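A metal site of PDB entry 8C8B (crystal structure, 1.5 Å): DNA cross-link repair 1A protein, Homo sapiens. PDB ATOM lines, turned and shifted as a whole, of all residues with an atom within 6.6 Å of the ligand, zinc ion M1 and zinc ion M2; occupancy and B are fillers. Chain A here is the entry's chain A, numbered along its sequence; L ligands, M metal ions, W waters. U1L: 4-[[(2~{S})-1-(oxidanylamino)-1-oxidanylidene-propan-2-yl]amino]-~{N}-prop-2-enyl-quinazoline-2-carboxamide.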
ATOM      1  N   HIS A  35       2.771  -0.421 -24.205  1.00  0.00           N
ATOM      2  CA  HIS A  35       2.000  -1.567 -23.751  1.00  0.00           C
ATOM      3  C   HIS A  35       1.414  -2.307 -24.949  1.00  0.00           C
ATOM      4  O   HIS A  35       1.370  -1.777 -26.062  1.00  0.00           O
ATOM      5  CB  HIS A  35       0.899  -1.170 -22.761  1.00  0.00           C
ATOM      6  CG  HIS A  35      -0.195  -0.322 -23.337  1.00  0.00           C
ATOM      7  ND1 HIS A  35       0.005   0.968 -23.779  1.00  0.00           N
ATOM      8  CD2 HIS A  35      -1.513  -0.561 -23.480  1.00  0.00           C
ATOM      9  CE1 HIS A  35      -1.138   1.474 -24.183  1.00  0.00           C
ATOM     10  NE2 HIS A  35      -2.074   0.563 -24.025  1.00  0.00           N
ATOM     11  N   PHE A  36       0.952  -3.536 -24.690  1.00  0.00           N
ATOM     12  CA  PHE A  36       0.518  -4.453 -25.745  1.00  0.00           C
ATOM     13  C   PHE A  36      -0.992  -4.324 -25.980  1.00  0.00           C
ATOM     14  O   PHE A  36      -1.801  -5.212 -25.667  1.00  0.00           O
ATOM     15  CB  PHE A  36       0.919  -5.887 -25.395  1.00  0.00           C
ATOM     16  CG  PHE A  36       0.778  -6.869 -26.536  1.00  0.00           C
ATOM     17  CD1 PHE A  36       1.717  -6.906 -27.555  1.00  0.00           C
ATOM     18  CD2 PHE A  36      -0.285  -7.753 -26.582  1.00  0.00           C
ATOM     19  CE1 PHE A  36       1.598  -7.810 -28.598  1.00  0.00           C
ATOM     20  CE2 PHE A  36      -0.428  -8.651 -27.624  1.00  0.00           C
ATOM     21  CZ  PHE A  36       0.524  -8.687 -28.638  1.00  0.00           C
ATOM     22  N   HIS A  37      -1.378  -3.162 -26.512  1.00  0.00           N
ATOM     23  CA  HIS A  37      -2.733  -2.935 -27.006  1.00  0.00           C
ATOM     24  C   HIS A  37      -2.642  -2.560 -28.475  1.00  0.00           C
ATOM     25  O   HIS A  37      -1.753  -1.794 -28.882  1.00  0.00           O
ATOM     26  CB  HIS A  37      -3.442  -1.840 -26.215  1.00  0.00           C
ATOM     27  CG  HIS A  37      -4.082  -2.335 -24.951  1.00  0.00           C
ATOM     28  ND1 HIS A  37      -4.446  -1.493 -23.926  1.00  0.00           N
ATOM     29  CD2 HIS A  37      -4.423  -3.581 -24.550  1.00  0.00           C
ATOM     30  CE1 HIS A  37      -4.998  -2.186 -22.946  1.00  0.00           C
ATOM     31  NE2 HIS A  37      -4.996  -3.461 -23.302  1.00  0.00           N
ATOM     32  N   SER A  38      -3.567  -3.107 -29.274  1.00  0.00           N
ATOM     33  CA  SER A  38      -3.424  -3.077 -30.729  1.00  0.00           C
ATOM     34  C   SER A  38      -3.305  -1.665 -31.286  1.00  0.00           C
ATOM     35  O   SER A  38      -2.579  -1.449 -32.256  1.00  0.00           O
ATOM     36  CB  SER A  38      -4.563  -3.842 -31.401  1.00  0.00           C
ATOM     37  OG  SER A  38      -5.815  -3.234 -31.158  1.00  0.00           O
ATOM     38  N   ASP A  39      -4.008  -0.696 -30.689  1.00  0.00           N
ATOM     39  CA  ASP A  39      -3.879   0.682 -31.166  1.00  0.00           C
ATOM     40  C   ASP A  39      -2.492   1.267 -30.938  1.00  0.00           C
ATOM     41  O   ASP A  39      -2.185   2.337 -31.476  1.00  0.00           O
ATOM     42  CB  ASP A  39      -4.975   1.597 -30.606  1.00  0.00           C
ATOM     43  CG  ASP A  39      -5.195   1.412 -29.112  1.00  0.00           C
ATOM     44  OD1 ASP A  39      -5.205   0.253 -28.642  1.00  0.00           O
ATOM     45  OD2 ASP A  39      -5.373   2.432 -28.407  1.00  0.00           O
ATOM     46  N   HIS A  40      -1.633   0.590 -30.180  1.00  0.00           N
ATOM     47  CA  HIS A  40      -0.262   1.046 -29.937  1.00  0.00           C
ATOM     48  C   HIS A  40       0.796   0.223 -30.635  1.00  0.00           C
ATOM     49  O   HIS A  40       1.798   0.789 -31.084  1.00  0.00           O
ATOM     50  CB  HIS A  40       0.028   1.073 -28.430  1.00  0.00           C
ATOM     51  CG  HIS A  40      -0.918   1.937 -27.679  1.00  0.00           C
ATOM     52  ND1 HIS A  40      -0.541   3.148 -27.128  1.00  0.00           N
ATOM     53  CD2 HIS A  40      -2.238   1.810 -27.444  1.00  0.00           C
ATOM     54  CE1 HIS A  40      -1.597   3.707 -26.560  1.00  0.00           C
ATOM     55  NE2 HIS A  40      -2.631   2.917 -26.742  1.00  0.00           N
ATOM     56  N   HIS A  96      -2.247   0.541 -15.958  1.00  0.00           N
ATOM     57  CA  HIS A  96      -3.164   0.370 -17.084  1.00  0.00           C
ATOM     58  C   HIS A  96      -3.426  -1.124 -17.200  1.00  0.00           C
ATOM     59  O   HIS A  96      -4.109  -1.691 -16.344  1.00  0.00           O
ATOM     60  CB  HIS A  96      -2.546   1.041 -18.317  1.00  0.00           C
ATOM     61  CG  HIS A  96      -3.408   1.012 -19.541  1.00  0.00           C
ATOM     62  ND1 HIS A  96      -4.695   1.504 -19.582  1.00  0.00           N
ATOM     63  CD2 HIS A  96      -3.146   0.546 -20.785  1.00  0.00           C
ATOM     64  CE1 HIS A  96      -5.190   1.341 -20.789  1.00  0.00           C
ATOM     65  NE2 HIS A  96      -4.268   0.750 -21.532  1.00  0.00           N
ATOM     66  N   CYS A  97      -2.857  -1.791 -18.187  1.00  0.00           N
ATOM     67  CA  CYS A  97      -2.949  -3.240 -18.321  1.00  0.00           C
ATOM     68  C   CYS A  97      -1.603  -3.875 -17.969  1.00  0.00           C
ATOM     69  O   CYS A  97      -0.612  -3.176 -17.734  1.00  0.00           O
ATOM     70  CB  CYS A  97      -3.339  -3.587 -19.763  1.00  0.00           C
ATOM     71  SG  CYS A  97      -2.068  -3.146 -20.967  1.00  0.00           S
ATOM     72  N   ASP A 118      -0.740   4.856 -22.069  1.00  0.00           N
ATOM     73  CA  ASP A 118      -2.046   4.838 -21.419  1.00  0.00           C
ATOM     74  C   ASP A 118      -1.851   4.593 -19.933  1.00  0.00           C
ATOM     75  O   ASP A 118      -1.046   3.749 -19.535  1.00  0.00           O
ATOM     76  CB  ASP A 118      -2.934   3.724 -21.980  1.00  0.00           C
ATOM     77  CG  ASP A 118      -3.472   4.019 -23.348  1.00  0.00           C
ATOM     78  OD1 ASP A 118      -3.291   5.167 -23.819  1.00  0.00           O
ATOM     79  OD2 ASP A 118      -4.075   3.095 -23.939  1.00  0.00           O
ATOM     80  N   ASP A 141      -2.036  10.898 -21.454  1.00  0.00           N
ATOM     81  CA  ASP A 141      -3.219  10.131 -21.841  1.00  0.00           C
ATOM     82  C   ASP A 141      -4.436  10.911 -21.384  1.00  0.00           C
ATOM     83  O   ASP A 141      -4.796  10.894 -20.194  1.00  0.00           O
ATOM     84  CB  ASP A 141      -3.158   8.746 -21.208  1.00  0.00           C
ATOM     85  CG  ASP A 141      -4.465   7.966 -21.318  1.00  0.00           C
ATOM     86  OD1 ASP A 141      -5.342   8.357 -22.111  1.00  0.00           O
ATOM     87  OD2 ASP A 141      -4.617   6.977 -20.577  1.00  0.00           O
ATOM     88  N   THR A 143      -7.611  10.444 -22.374  1.00  0.00           N
ATOM     89  CA  THR A 143      -8.809   9.727 -22.815  1.00  0.00           C
ATOM     90  C   THR A 143     -10.073  10.326 -22.214  1.00  0.00           C
ATOM     91  O   THR A 143     -11.048  10.590 -22.921  1.00  0.00           O
ATOM     92  CB  THR A 143      -8.696   8.232 -22.473  1.00  0.00           C
ATOM     93  OG1 THR A 143      -7.609   7.660 -23.211  1.00  0.00           O
ATOM     94  CG2 THR A 143      -9.975   7.485 -22.835  1.00  0.00           C
ATOM     95  N   TYR A 144     -10.077  10.556 -20.904  1.00  0.00           N
ATOM     96  CA  TYR A 144     -11.262  11.010 -20.179  1.00  0.00           C
ATOM     97  C   TYR A 144     -11.063  12.395 -19.571  1.00  0.00           C
ATOM     98  O   TYR A 144     -11.454  12.672 -18.432  1.00  0.00           O
ATOM     99  CB  TYR A 144     -11.655  10.004 -19.096  1.00  0.00           C
ATOM    100  CG  TYR A 144     -12.151   8.689 -19.649  1.00  0.00           C
ATOM    101  CD1 TYR A 144     -13.145   8.649 -20.614  1.00  0.00           C
ATOM    102  CD2 TYR A 144     -11.620   7.476 -19.201  1.00  0.00           C
ATOM    103  CE1 TYR A 144     -13.613   7.442 -21.113  1.00  0.00           C
ATOM    104  CE2 TYR A 144     -12.071   6.284 -19.705  1.00  0.00           C
ATOM    105  CZ  TYR A 144     -13.066   6.271 -20.655  1.00  0.00           C
ATOM    106  OH  TYR A 144     -13.516   5.065 -21.139  1.00  0.00           O
ATOM    107  N   TYR A 182     -11.492  -8.628 -24.867  1.00  0.00           N
ATOM    108  CA  TYR A 182     -10.988  -8.459 -26.228  1.00  0.00           C
ATOM    109  C   TYR A 182      -9.499  -8.144 -26.320  1.00  0.00           C
ATOM    110  O   TYR A 182      -8.950  -8.152 -27.422  1.00  0.00           O
ATOM    111  CB  TYR A 182     -11.782  -7.410 -27.028  1.00  0.00           C
ATOM    112  CG  TYR A 182     -12.019  -6.089 -26.328  1.00  0.00           C
ATOM    113  CD1 TYR A 182     -10.965  -5.326 -25.827  1.00  0.00           C
ATOM    114  CD2 TYR A 182     -13.304  -5.565 -26.212  1.00  0.00           C
ATOM    115  CE1 TYR A 182     -11.188  -4.111 -25.212  1.00  0.00           C
ATOM    116  CE2 TYR A 182     -13.536  -4.352 -25.593  1.00  0.00           C
ATOM    117  CZ  TYR A 182     -12.484  -3.630 -25.096  1.00  0.00           C
ATOM    118  OH  TYR A 182     -12.705  -2.424 -24.482  1.00  0.00           O
ATOM    119  N   SER A 183      -8.836  -7.862 -25.198  1.00  0.00           N
ATOM    120  CA  SER A 183      -7.407  -7.560 -25.175  1.00  0.00           C
ATOM    121  C   SER A 183      -6.924  -7.891 -23.776  1.00  0.00           C
ATOM    122  O   SER A 183      -7.700  -8.311 -22.916  1.00  0.00           O
ATOM    123  CB  SER A 183      -7.182  -6.081 -25.497  1.00  0.00           C
ATOM    124  OG  SER A 183      -7.942  -5.259 -24.625  1.00  0.00           O
ATOM    125  N   ILE A 184      -5.622  -7.695 -23.541  1.00  0.00           N
ATOM    126  CA  ILE A 184      -5.159  -7.786 -22.171  1.00  0.00           C
ATOM    127  C   ILE A 184      -5.676  -6.597 -21.369  1.00  0.00           C
ATOM    128  O   ILE A 184      -6.130  -5.588 -21.920  1.00  0.00           O
ATOM    129  CB  ILE A 184      -3.626  -7.893 -22.077  1.00  0.00           C
ATOM    130  CG1 ILE A 184      -2.963  -6.618 -22.599  1.00  0.00           C
ATOM    131  CG2 ILE A 184      -3.129  -9.132 -22.798  1.00  0.00           C
ATOM    132  CD1 ILE A 184      -1.476  -6.542 -22.264  1.00  0.00           C
ATOM    133  N   LYS A 186      -7.815  -5.760 -17.380  1.00  0.00           N
ATOM    134  CA  LYS A 186      -9.068  -6.055 -16.697  1.00  0.00           C
ATOM    135  C   LYS A 186      -9.183  -7.506 -16.257  1.00  0.00           C
ATOM    136  O   LYS A 186     -10.280  -7.984 -15.976  1.00  0.00           O
ATOM    137  CB  LYS A 186     -10.286  -5.596 -17.514  1.00  0.00           C
ATOM    138  CG  LYS A 186     -10.112  -4.179 -18.096  1.00  0.00           C
ATOM    139  CD  LYS A 186     -11.366  -3.641 -18.766  1.00  0.00           C
ATOM    140  CE  LYS A 186     -11.090  -2.268 -19.400  1.00  0.00           C
ATOM    141  NZ  LYS A 186     -12.344  -1.582 -19.821  1.00  0.00           N
ATOM    142  N   GLY A 266     -15.658   0.787 -20.525  1.00  0.00           N
ATOM    143  CA  GLY A 266     -15.001   1.956 -19.974  1.00  0.00           C
ATOM    144  C   GLY A 266     -16.012   2.817 -19.271  1.00  0.00           C
ATOM    145  O   GLY A 266     -16.836   2.313 -18.499  1.00  0.00           O
ATOM    146  N   TRP A 267     -15.976   4.123 -19.515  1.00  0.00           N
ATOM    147  CA  TRP A 267     -16.990   5.017 -18.984  1.00  0.00           C
ATOM    148  C   TRP A 267     -18.252   4.925 -19.821  1.00  0.00           C
ATOM    149  O   TRP A 267     -18.201   4.789 -21.043  1.00  0.00           O
ATOM    150  CB  TRP A 267     -16.482   6.457 -19.008  1.00  0.00           C
ATOM    151  CG  TRP A 267     -17.561   7.488 -18.807  1.00  0.00           C
ATOM    152  CD1 TRP A 267     -17.988   8.018 -17.623  1.00  0.00           C
ATOM    153  CD2 TRP A 267     -18.353   8.115 -19.833  1.00  0.00           C
ATOM    154  NE1 TRP A 267     -18.994   8.937 -17.844  1.00  0.00           N
ATOM    155  CE2 TRP A 267     -19.234   9.013 -19.196  1.00  0.00           C
ATOM    156  CE3 TRP A 267     -18.403   7.996 -21.227  1.00  0.00           C
ATOM    157  CZ2 TRP A 267     -20.152   9.784 -19.905  1.00  0.00           C
ATOM    158  CZ3 TRP A 267     -19.308   8.768 -21.931  1.00  0.00           C
ATOM    159  CH2 TRP A 267     -20.174   9.653 -21.269  1.00  0.00           C
ATOM    160  N   GLU A 296      -9.361   1.225 -17.008  1.00  0.00           N
ATOM    161  CA  GLU A 296      -7.904   1.294 -16.880  1.00  0.00           C
ATOM    162  C   GLU A 296      -7.327   2.614 -17.392  1.00  0.00           C
ATOM    163  O   GLU A 296      -6.126   2.701 -17.643  1.00  0.00           O
ATOM    164  CB  GLU A 296      -7.231   0.043 -17.485  1.00  0.00           C
ATOM    165  CG  GLU A 296      -7.468  -1.182 -16.565  1.00  0.00           C
ATOM    166  CD  GLU A 296      -6.862  -2.490 -17.046  1.00  0.00           C
ATOM    167  OE1 GLU A 296      -6.485  -2.607 -18.226  1.00  0.00           O
ATOM    168  OE2 GLU A 296      -6.761  -3.423 -16.203  1.00  0.00           O
ATOM    169  N   HIS A 297      -8.172   3.644 -17.508  1.00  0.00           N
ATOM    170  CA  HIS A 297      -7.731   5.008 -17.787  1.00  0.00           C
ATOM    171  C   HIS A 297      -8.145   5.909 -16.633  1.00  0.00           C
ATOM    172  O   HIS A 297      -9.152   5.640 -15.961  1.00  0.00           O
ATOM    173  CB  HIS A 297      -8.370   5.578 -19.066  1.00  0.00           C
ATOM    174  CG  HIS A 297      -7.938   4.889 -20.336  1.00  0.00           C
ATOM    175  ND1 HIS A 297      -6.778   5.217 -21.006  1.00  0.00           N
ATOM    176  CD2 HIS A 297      -8.523   3.901 -21.054  1.00  0.00           C
ATOM    177  CE1 HIS A 297      -6.664   4.452 -22.073  1.00  0.00           C
ATOM    178  NE2 HIS A 297      -7.708   3.646 -22.130  1.00  0.00           N
ATOM    179  N   VAL A 319      -4.507  11.784 -26.723  1.00  0.00           N
ATOM    180  CA  VAL A 319      -5.826  11.223 -27.014  1.00  0.00           C
ATOM    181  C   VAL A 319      -6.808  12.366 -27.198  1.00  0.00           C
ATOM    182  O   VAL A 319      -6.683  13.425 -26.571  1.00  0.00           O
ATOM    183  CB  VAL A 319      -6.319  10.238 -25.917  1.00  0.00           C
ATOM    184  CG1 VAL A 319      -7.629   9.522 -26.306  1.00  0.00           C
ATOM    185  CG2 VAL A 319      -5.251   9.193 -25.628  1.00  0.00           C
HETATM  186  C1  U1L L   1      -8.052  -1.928 -24.517  1.00  0.00           C
HETATM  187  C10 U1L L   1      -9.126   1.374 -29.542  1.00  0.00           C
HETATM  188  C11 U1L L   1      -9.461   2.436 -27.501  1.00  0.00           C
HETATM  189  C12 U1L L   1      -9.934   3.637 -26.773  1.00  0.00           C
HETATM  190  C13 U1L L   1     -10.874   3.806 -24.523  1.00  0.00           C
HETATM  191  C14 U1L L   1     -11.796   4.911 -24.827  1.00  0.00           C
HETATM  192  C15 U1L L   1     -13.054   4.810 -25.137  1.00  0.00           C
HETATM  193  C2  U1L L   1      -8.020  -0.600 -25.254  1.00  0.00           C
HETATM  194  C3  U1L L   1      -6.772   0.192 -24.883  1.00  0.00           C
HETATM  195  C4  U1L L   1      -8.596   0.293 -27.443  1.00  0.00           C
HETATM  196  C5  U1L L   1      -8.633   0.226 -28.881  1.00  0.00           C
HETATM  197  C6  U1L L   1      -8.209  -0.884 -29.643  1.00  0.00           C
HETATM  198  C7  U1L L   1      -8.274  -0.848 -31.002  1.00  0.00           C
HETATM  199  C8  U1L L   1      -8.763   0.299 -31.654  1.00  0.00           C
HETATM  200  C9  U1L L   1      -9.182   1.380 -30.953  1.00  0.00           C
HETATM  201  N1  U1L L   1      -5.882   0.403 -25.840  1.00  0.00           N
HETATM  202  N2  U1L L   1      -8.134  -0.768 -26.724  1.00  0.00           N
HETATM  203  N3  U1L L   1      -9.541   2.477 -28.841  1.00  0.00           N
HETATM  204  N4  U1L L   1      -9.763   3.657 -25.445  1.00  0.00           N
HETATM  205  N5  U1L L   1      -9.018   1.384 -26.794  1.00  0.00           N
HETATM  206  O1  U1L L   1      -4.727   1.135 -25.567  1.00  0.00           O
HETATM  207  O2  U1L L   1      -6.629   0.615 -23.740  1.00  0.00           O
HETATM  208  O3  U1L L   1     -10.520   4.532 -27.387  1.00  0.00           O
HETATM  209 ZN    ZN M   1      -4.256   0.706 -23.731  1.00  0.00          ZN
HETATM  210 ZN    ZN M   2      -4.712   3.086 -25.960  1.00  0.00          ZN
HETATM  211  O   HOH W   1      -4.788   5.145 -25.923  1.00  0.00           O
HETATM  212  O   HOH W   2      -6.855   3.124 -25.142  1.00  0.00           O
HETATM  213  O   HOH W   3      -7.452   5.982 -25.496  1.00  0.00           O
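OD1 of Asp 39 lies within hydrogen-bond range of N1 of the ligand (2.9 Å).
NE2 of His 40 lies close to OD2 of Asp 39 (3.2 Å). OD1 of Asp 141 sits at hydrogen-bond distance from OG1 of Thr 143 (2.6 Å). The side-chain carboxylate (OD2) of Asp 141 is in hydrogen-bond range of a ring nitrogen (ND1) of His 297, at 2.8 Å. ND1 of His 297 lies within hydrogen-bond range of OG1 of Thr 143 (3.4 Å). NE2 of His 37 lies close to SG of Cys 97 (3.8 Å). The backbone carbonyl oxygen (O) of Glu 296 is in hydrogen-bond range of a ring nitrogen (ND1) of His 96 (2.7 Å). O of Ile 184 is in hydrogen-bond range of NE2 of His 37 (2.8 Å).
Merely in contact with the ligand: Ser 183, Ser 38, His 297, Thr 143 and Tyr 182. Hydrophobic or aromatic side chains that line the ligand: His 35, His 37, His 40, His 96 and Tyr 182. 11 residues have an atom within 4 Å of the ligand: His 35, His 37, Ser 38, Asp 39, His 40, His 96, Asp 118, Thr 143, Tyr 182, Ser 183 and His 297. The nearest printed residue that does not touch the ligand is Tyr 144 (4.03 Å).
Along chain A the residues within 4 Å of zinc ion M1 span positions 35 to 118.
Along chain A the residues within 4 Å of zinc ion M2 span positions 39 to 118. The nearest printed residue that does not touch zinc ion M2 is His 35 (4.1 Å).
Zinc ion M1 is bound by O1 of the ligand (1.9 Å), NE2 of His 96 (2.2 Å), NE2 of His 35 (2.2 Å), ND1 of His 37 (2.2 Å), O2 of the ligand (2.4 Å) and OD2 of Asp 118 (2.4 Å). Zinc ion M1 has six donor atoms within binding distance.
Zinc ion M2 is bound by O1 of the ligand (2.0 Å), water W1 (2.1 Å), OD2 of Asp 118 (2.1 Å), NE2 of His 40 (2.2 Å) and water W2 (2.3 Å). Zinc ion M2 has five donor atoms within binding distance. Slightly farther from zinc ion M2 lies OD2 of Asp 39 (2.6 Å).
Water W2 bridges N4 of the ligand and NE2 of His 297. Water W3 lies within hydrogen-bond range of the side-chain hydroxyl of Thr 143 and a nitrogen (N4) of the ligand.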
